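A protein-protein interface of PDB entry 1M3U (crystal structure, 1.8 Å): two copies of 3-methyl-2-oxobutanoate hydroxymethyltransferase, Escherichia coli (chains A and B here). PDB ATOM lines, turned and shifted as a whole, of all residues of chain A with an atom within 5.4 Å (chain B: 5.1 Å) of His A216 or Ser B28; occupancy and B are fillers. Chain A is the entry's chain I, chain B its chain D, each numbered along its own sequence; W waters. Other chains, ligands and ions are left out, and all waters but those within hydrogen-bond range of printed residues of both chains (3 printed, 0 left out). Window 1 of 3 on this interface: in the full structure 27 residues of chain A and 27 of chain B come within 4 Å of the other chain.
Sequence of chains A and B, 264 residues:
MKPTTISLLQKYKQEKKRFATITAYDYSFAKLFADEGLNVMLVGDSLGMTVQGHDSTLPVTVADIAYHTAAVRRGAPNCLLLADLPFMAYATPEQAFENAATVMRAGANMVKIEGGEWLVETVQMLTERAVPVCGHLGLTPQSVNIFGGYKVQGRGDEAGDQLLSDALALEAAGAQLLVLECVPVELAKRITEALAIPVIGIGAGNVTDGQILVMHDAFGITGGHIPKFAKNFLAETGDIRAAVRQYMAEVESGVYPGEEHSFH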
ATOM      1  N   THR A  23      38.652   1.687 -19.603  1.00  0.00           N
ATOM      2  CA  THR A  23      37.949   0.988 -20.656  1.00  0.00           C
ATOM      3  C   THR A  23      38.006   1.805 -21.953  1.00  0.00           C
ATOM      4  O   THR A  23      38.150   3.030 -21.949  1.00  0.00           O
ATOM      5  CB  THR A  23      36.489   0.704 -20.315  1.00  0.00           C
ATOM      6  OG1 THR A  23      35.768   1.929 -20.314  1.00  0.00           O
ATOM      7  CG2 THR A  23      36.322   0.024 -18.898  1.00  0.00           C
ATOM      8  N   TYR A  25      36.399   1.356 -26.279  1.00  0.00           N
ATOM      9  CA  TYR A  25      35.564   0.572 -27.186  1.00  0.00           C
ATOM     10  C   TYR A  25      35.609   1.011 -28.643  1.00  0.00           C
ATOM     11  O   TYR A  25      34.899   0.446 -29.476  1.00  0.00           O
ATOM     12  CB  TYR A  25      34.099   0.545 -26.701  1.00  0.00           C
ATOM     13  CG  TYR A  25      33.917   0.459 -25.189  1.00  0.00           C
ATOM     14  CD1 TYR A  25      33.596   1.593 -24.444  1.00  0.00           C
ATOM     15  CD2 TYR A  25      34.059  -0.757 -24.509  1.00  0.00           C
ATOM     16  CE1 TYR A  25      33.419   1.538 -23.080  1.00  0.00           C
ATOM     17  CE2 TYR A  25      33.889  -0.818 -23.112  1.00  0.00           C
ATOM     18  CZ  TYR A  25      33.559   0.346 -22.430  1.00  0.00           C
ATOM     19  OH  TYR A  25      33.365   0.310 -21.102  1.00  0.00           O
ATOM     20  N   MET A  49      26.186  -1.870 -21.756  1.00  0.00           N
ATOM     21  CA  MET A  49      25.369  -0.816 -21.180  1.00  0.00           C
ATOM     22  C   MET A  49      25.738   0.544 -21.757  1.00  0.00           C
ATOM     23  O   MET A  49      24.892   1.202 -22.286  1.00  0.00           O
ATOM     24  CB  MET A  49      25.499  -0.850 -19.646  1.00  0.00           C
ATOM     25  CG  MET A  49      25.073  -2.176 -19.085  1.00  0.00           C
ATOM     26  SD  MET A  49      25.182  -2.386 -17.285  1.00  0.00           S
ATOM     27  CE  MET A  49      24.022  -1.280 -16.723  1.00  0.00           C
ATOM     28  N   THR A  50      27.014   0.925 -21.698  1.00  0.00           N
ATOM     29  CA  THR A  50      27.448   2.278 -22.067  1.00  0.00           C
ATOM     30  C   THR A  50      27.444   2.490 -23.580  1.00  0.00           C
ATOM     31  O   THR A  50      27.142   3.572 -24.049  1.00  0.00           O
ATOM     32  CB  THR A  50      28.857   2.560 -21.523  1.00  0.00           C
ATOM     33  OG1 THR A  50      29.767   1.678 -22.160  1.00  0.00           O
ATOM     34  CG2 THR A  50      28.948   2.181 -20.085  1.00  0.00           C
ATOM     35  N   VAL A  51      27.679   1.414 -24.335  1.00  0.00           N
ATOM     36  CA  VAL A  51      27.692   1.485 -25.792  1.00  0.00           C
ATOM     37  C   VAL A  51      26.374   1.020 -26.395  1.00  0.00           C
ATOM     38  O   VAL A  51      25.722   1.791 -27.176  1.00  0.00           O
ATOM     39  CB  VAL A  51      28.889   0.716 -26.372  1.00  0.00           C
ATOM     40  CG1 VAL A  51      28.819   0.663 -27.934  1.00  0.00           C
ATOM     41  CG2 VAL A  51      30.165   1.327 -25.912  1.00  0.00           C
ATOM     42  N   VAL A 214      35.289   2.977 -16.221  1.00  0.00           N
ATOM     43  CA  VAL A 214      34.633   3.095 -17.513  1.00  0.00           C
ATOM     44  C   VAL A 214      34.884   4.526 -17.993  1.00  0.00           C
ATOM     45  O   VAL A 214      34.620   5.509 -17.302  1.00  0.00           O
ATOM     46  CB  VAL A 214      33.099   2.760 -17.450  1.00  0.00           C
ATOM     47  CG1 VAL A 214      32.376   3.211 -18.706  1.00  0.00           C
ATOM     48  CG2 VAL A 214      32.856   1.227 -17.159  1.00  0.00           C
ATOM     49  N   MET A 215      35.430   4.643 -19.190  1.00  0.00           N
ATOM     50  CA  MET A 215      35.785   5.973 -19.685  1.00  0.00           C
ATOM     51  C   MET A 215      34.592   6.933 -19.775  1.00  0.00           C
ATOM     52  O   MET A 215      34.772   8.138 -19.675  1.00  0.00           O
ATOM     53  CB  MET A 215      36.494   5.870 -21.028  1.00  0.00           C
ATOM     54  CG  MET A 215      35.688   5.146 -22.115  1.00  0.00           C
ATOM     55  SD  MET A 215      35.892   5.987 -23.710  1.00  0.00           S
ATOM     56  CE  MET A 215      34.867   7.385 -23.405  1.00  0.00           C
ATOM     57  N   HIS A 216      33.372   6.436 -19.961  1.00  0.00           N
ATOM     58  CA  HIS A 216      32.212   7.339 -20.087  1.00  0.00           C
ATOM     59  C   HIS A 216      31.892   8.047 -18.766  1.00  0.00           C
ATOM     60  O   HIS A 216      31.422   9.193 -18.755  1.00  0.00           O
ATOM     61  CB  HIS A 216      30.992   6.614 -20.690  1.00  0.00           C
ATOM     62  CG  HIS A 216      31.222   6.169 -22.113  1.00  0.00           C
ATOM     63  ND1 HIS A 216      32.015   5.087 -22.438  1.00  0.00           N
ATOM     64  CD2 HIS A 216      30.851   6.727 -23.289  1.00  0.00           C
ATOM     65  CE1 HIS A 216      32.057   4.958 -23.754  1.00  0.00           C
ATOM     66  NE2 HIS A 216      31.370   5.947 -24.298  1.00  0.00           N
ATOM     67  N   ASP A 217      32.170   7.368 -17.662  1.00  0.00           N
ATOM     68  CA  ASP A 217      32.026   7.965 -16.349  1.00  0.00           C
ATOM     69  C   ASP A 217      33.160   8.956 -16.110  1.00  0.00           C
ATOM     70  O   ASP A 217      32.936  10.010 -15.598  1.00  0.00           O
ATOM     71  CB  ASP A 217      32.065   6.871 -15.273  1.00  0.00           C
ATOM     72  CG  ASP A 217      30.936   5.882 -15.411  1.00  0.00           C
ATOM     73  OD1 ASP A 217      29.811   6.308 -15.806  1.00  0.00           O
ATOM     74  OD2 ASP A 217      31.115   4.655 -15.198  1.00  0.00           O
ATOM     75  N   ALA A 218      34.374   8.598 -16.515  1.00  0.00           N
ATOM     76  CA  ALA A 218      35.555   9.415 -16.219  1.00  0.00           C
ATOM     77  C   ALA A 218      35.544  10.723 -16.913  1.00  0.00           C
ATOM     78  O   ALA A 218      35.959  11.743 -16.357  1.00  0.00           O
ATOM     79  CB  ALA A 218      36.822   8.686 -16.562  1.00  0.00           C
ATOM     80  N   PHE A 219      35.087  10.736 -18.143  1.00  0.00           N
ATOM     81  CA  PHE A 219      35.363  11.882 -18.963  1.00  0.00           C
ATOM     82  C   PHE A 219      34.089  12.596 -19.256  1.00  0.00           C
ATOM     83  O   PHE A 219      34.004  13.208 -20.289  1.00  0.00           O
ATOM     84  CB  PHE A 219      36.196  11.512 -20.228  1.00  0.00           C
ATOM     85  CG  PHE A 219      37.507  10.835 -19.879  1.00  0.00           C
ATOM     86  CD1 PHE A 219      37.793   9.556 -20.340  1.00  0.00           C
ATOM     87  CD2 PHE A 219      38.387  11.426 -18.997  1.00  0.00           C
ATOM     88  CE1 PHE A 219      38.973   8.887 -19.945  1.00  0.00           C
ATOM     89  CE2 PHE A 219      39.581  10.759 -18.579  1.00  0.00           C
ATOM     90  CZ  PHE A 219      39.874   9.491 -19.071  1.00  0.00           C
ATOM     91  N   GLY A 220      33.128  12.519 -18.319  1.00  0.00           N
ATOM     92  CA  GLY A 220      31.938  13.359 -18.298  1.00  0.00           C
ATOM     93  C   GLY A 220      30.792  13.114 -19.250  1.00  0.00           C
ATOM     94  O   GLY A 220      30.119  14.082 -19.630  1.00  0.00           O
ATOM     95  N   ILE A 221      30.554  11.861 -19.648  1.00  0.00           N
ATOM     96  CA  ILE A 221      29.558  11.567 -20.692  1.00  0.00           C
ATOM     97  C   ILE A 221      28.317  10.942 -20.117  1.00  0.00           C
ATOM     98  O   ILE A 221      27.228  11.197 -20.535  1.00  0.00           O
ATOM     99  CB  ILE A 221      30.182  10.642 -21.735  1.00  0.00           C
ATOM    100  CG1 ILE A 221      31.428  11.313 -22.340  1.00  0.00           C
ATOM    101  CG2 ILE A 221      29.134  10.215 -22.790  1.00  0.00           C
ATOM    102  CD1 ILE A 221      32.493  10.306 -22.806  1.00  0.00           C
ATOM    103  N   THR A 222      28.499  10.090 -19.125  1.00  0.00           N
ATOM    104  CA  THR A 222      27.385   9.389 -18.542  1.00  0.00           C
ATOM    105  C   THR A 222      26.432  10.355 -17.848  1.00  0.00           C
ATOM    106  O   THR A 222      26.869  11.288 -17.237  1.00  0.00           O
ATOM    107  CB  THR A 222      27.926   8.320 -17.574  1.00  0.00           C
ATOM    108  OG1 THR A 222      28.510   7.287 -18.376  1.00  0.00           O
ATOM    109  CG2 THR A 222      26.784   7.638 -16.817  1.00  0.00           C
ATOM    110  N   ASP B  26      26.555   5.408 -30.453  1.00  0.00           N
ATOM    111  CA  ASP B  26      26.401   4.641 -29.237  1.00  0.00           C
ATOM    112  C   ASP B  26      25.349   5.227 -28.333  1.00  0.00           C
ATOM    113  O   ASP B  26      24.908   6.349 -28.527  1.00  0.00           O
ATOM    114  CB  ASP B  26      27.731   4.526 -28.495  1.00  0.00           C
ATOM    115  CG  ASP B  26      28.279   5.842 -28.025  1.00  0.00           C
ATOM    116  OD1 ASP B  26      27.779   6.382 -27.026  1.00  0.00           O
ATOM    117  OD2 ASP B  26      29.239   6.434 -28.577  1.00  0.00           O
ATOM    118  N   TYR B  27      24.973   4.445 -27.331  1.00  0.00           N
ATOM    119  CA  TYR B  27      23.914   4.807 -26.403  1.00  0.00           C
ATOM    120  C   TYR B  27      24.238   6.055 -25.596  1.00  0.00           C
ATOM    121  O   TYR B  27      23.378   6.925 -25.404  1.00  0.00           O
ATOM    122  CB  TYR B  27      23.648   3.616 -25.472  1.00  0.00           C
ATOM    123  CG  TYR B  27      22.810   3.988 -24.255  1.00  0.00           C
ATOM    124  CD1 TYR B  27      21.421   3.887 -24.291  1.00  0.00           C
ATOM    125  CD2 TYR B  27      23.419   4.434 -23.074  1.00  0.00           C
ATOM    126  CE1 TYR B  27      20.658   4.240 -23.186  1.00  0.00           C
ATOM    127  CE2 TYR B  27      22.667   4.774 -21.972  1.00  0.00           C
ATOM    128  CZ  TYR B  27      21.280   4.661 -22.029  1.00  0.00           C
ATOM    129  OH  TYR B  27      20.521   4.992 -20.913  1.00  0.00           O
ATOM    130  N   SER B  28      25.471   6.170 -25.113  1.00  0.00           N
ATOM    131  CA  SER B  28      25.799   7.200 -24.135  1.00  0.00           C
ATOM    132  C   SER B  28      25.757   8.597 -24.750  1.00  0.00           C
ATOM    133  O   SER B  28      25.114   9.530 -24.219  1.00  0.00           O
ATOM    134  CB  SER B  28      27.156   6.929 -23.476  1.00  0.00           C
ATOM    135  OG  SER B  28      27.093   5.734 -22.680  1.00  0.00           O
ATOM    136  N   PHE B  29      26.391   8.748 -25.901  1.00  0.00           N
ATOM    137  CA  PHE B  29      26.338  10.041 -26.585  1.00  0.00           C
ATOM    138  C   PHE B  29      24.944  10.340 -27.118  1.00  0.00           C
ATOM    139  O   PHE B  29      24.491  11.478 -27.024  1.00  0.00           O
ATOM    140  CB  PHE B  29      27.407  10.122 -27.666  1.00  0.00           C
ATOM    141  CG  PHE B  29      28.775  10.477 -27.120  1.00  0.00           C
ATOM    142  CD1 PHE B  29      29.748   9.485 -26.948  1.00  0.00           C
ATOM    143  CD2 PHE B  29      29.064  11.776 -26.754  1.00  0.00           C
ATOM    144  CE1 PHE B  29      30.994   9.807 -26.455  1.00  0.00           C
ATOM    145  CE2 PHE B  29      30.297  12.105 -26.244  1.00  0.00           C
ATOM    146  CZ  PHE B  29      31.275  11.115 -26.098  1.00  0.00           C
ATOM    147  N   ALA B  30      24.245   9.321 -27.626  1.00  0.00           N
ATOM    148  CA  ALA B  30      22.902   9.539 -28.141  1.00  0.00           C
ATOM    149  C   ALA B  30      21.984  10.072 -27.010  1.00  0.00           C
ATOM    150  O   ALA B  30      21.249  11.050 -27.172  1.00  0.00           O
ATOM    151  CB  ALA B  30      22.341   8.307 -28.759  1.00  0.00           C
ATOM    152  N   LYS B  31      22.080   9.466 -25.839  1.00  0.00           N
ATOM    153  CA  LYS B  31      21.285   9.936 -24.707  1.00  0.00           C
ATOM    154  C   LYS B  31      21.635  11.356 -24.246  1.00  0.00           C
ATOM    155  O   LYS B  31      20.742  12.158 -23.919  1.00  0.00           O
ATOM    156  CB  LYS B  31      21.416   8.960 -23.554  1.00  0.00           C
ATOM    157  CG  LYS B  31      20.586   9.393 -22.324  1.00  0.00           C
ATOM    158  CD  LYS B  31      20.418   8.272 -21.334  1.00  0.00           C
ATOM    159  CE  LYS B  31      19.323   8.638 -20.303  1.00  0.00           C
ATOM    160  NZ  LYS B  31      18.056   9.045 -21.027  1.00  0.00           N
ATOM    161  N   LEU B  32      22.928  11.643 -24.126  1.00  0.00           N
ATOM    162  CA  LEU B  32      23.398  12.984 -23.820  1.00  0.00           C
ATOM    163  C   LEU B  32      22.797  14.022 -24.793  1.00  0.00           C
ATOM    164  O   LEU B  32      22.345  15.071 -24.383  1.00  0.00           O
ATOM    165  CB  LEU B  32      24.921  13.007 -23.879  1.00  0.00           C
ATOM    166  CG  LEU B  32      25.676  14.253 -23.384  1.00  0.00           C
ATOM    167  CD1 LEU B  32      27.115  13.899 -23.002  1.00  0.00           C
ATOM    168  CD2 LEU B  32      25.632  15.396 -24.395  1.00  0.00           C
HETATM  169  O   HOH W   1      24.853   9.785 -21.596  1.00  0.00           O
HETATM  170  O   HOH W   2      26.089   5.644 -20.277  1.00  0.00           O
HETATM  171  O   HOH W   3      31.386   6.348 -27.047  1.00  0.00           O
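N of Tyr B27 sits at hydrogen-bond distance from O of Val A51. OG of Ser B28 sits at hydrogen-bond distance from O of Thr A50 (2.6 Å).
The backbone NH (N) of Ser B28 lies within hydrogen-bond range of the side-chain carboxylate (OD1) of Asp B26. The side-chain carboxylate (OD1) of Asp B26 sits at hydrogen-bond distance from the backbone NH (N) of Phe B29 (3.0 Å). The backbone carbonyl oxygen (O) of His A216 sits at hydrogen-bond distance from the backbone NH (N) of Ile A221 (2.9 Å). The backbone NH (N) of Thr A222 sits at hydrogen-bond distance from the backbone carbonyl oxygen (O) of His A216 (3.1 Å).
Tyr B27 touches Met A49 (CD2 to O, 3.6 Å). CB of Tyr B27 touches O of Thr A50 (3.8 Å). Val A51 touches Asp B26. CD2 of His A216 touches CB of Ser B28, at 3.7 Å. CG2 of Ile A221 touches CB of Ser B28 (3.9 Å). Ile A221 touches Phe B29 (CD1 to CZ, 3.6 Å). O of Ile A221 touches CD1 of Leu B32 (3.7 Å).
Of the printed residues of chain B, Val A51 touches Asp B26 (3.6 Å) and Tyr B27 (2.8 Å). Of chain B, only Ser B28 (3.7 Å) comes within 4 Å of His A216. Asp A217 touches none of the printed residues of chain B. Ala A218 touches none of the printed residues of chain B. Ser B28 touches just these residues of chain A: Thr A50, His A216 and Ile A221. Of the printed residues of chain A, Phe B29 touches Ile A221.
Printed residues of chain B that touch a printed residue of chain A: Asp B26, Tyr B27, Ser B28, Phe B29 and Leu B32. Hydrophobic or aromatic side chains of chain B within 4 Å of the printed part of chain A: Tyr B27, Phe B29 and Leu B32. Along chain B the printed residues that touch a printed residue of chain A span positions 26 to 32. Hydrophobic or aromatic side chains of chain A within 4 Å of the printed part of chain B: His A216 and Ile A221.
No position is printed for both chains. Of the 9 pairs that touch across the chains among the printed residues, none has its exchanged pair printed and touching as well.
Water W2 lies within hydrogen-bond range of the side-chain hydroxyl (OG) of Ser B28 (2.6 Å) and the side-chain hydroxyl (OG1) of Thr A222 (3.5 Å). Water W3 lies within hydrogen-bond range of OD2 of Asp B26 (2.6 Å) and NE2 of His A216 (2.8 Å). Water W1 lies within hydrogen-bond range of the backbone carbonyl oxygen of Ser B28 and the backbone carbonyl oxygen of Ile A221.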
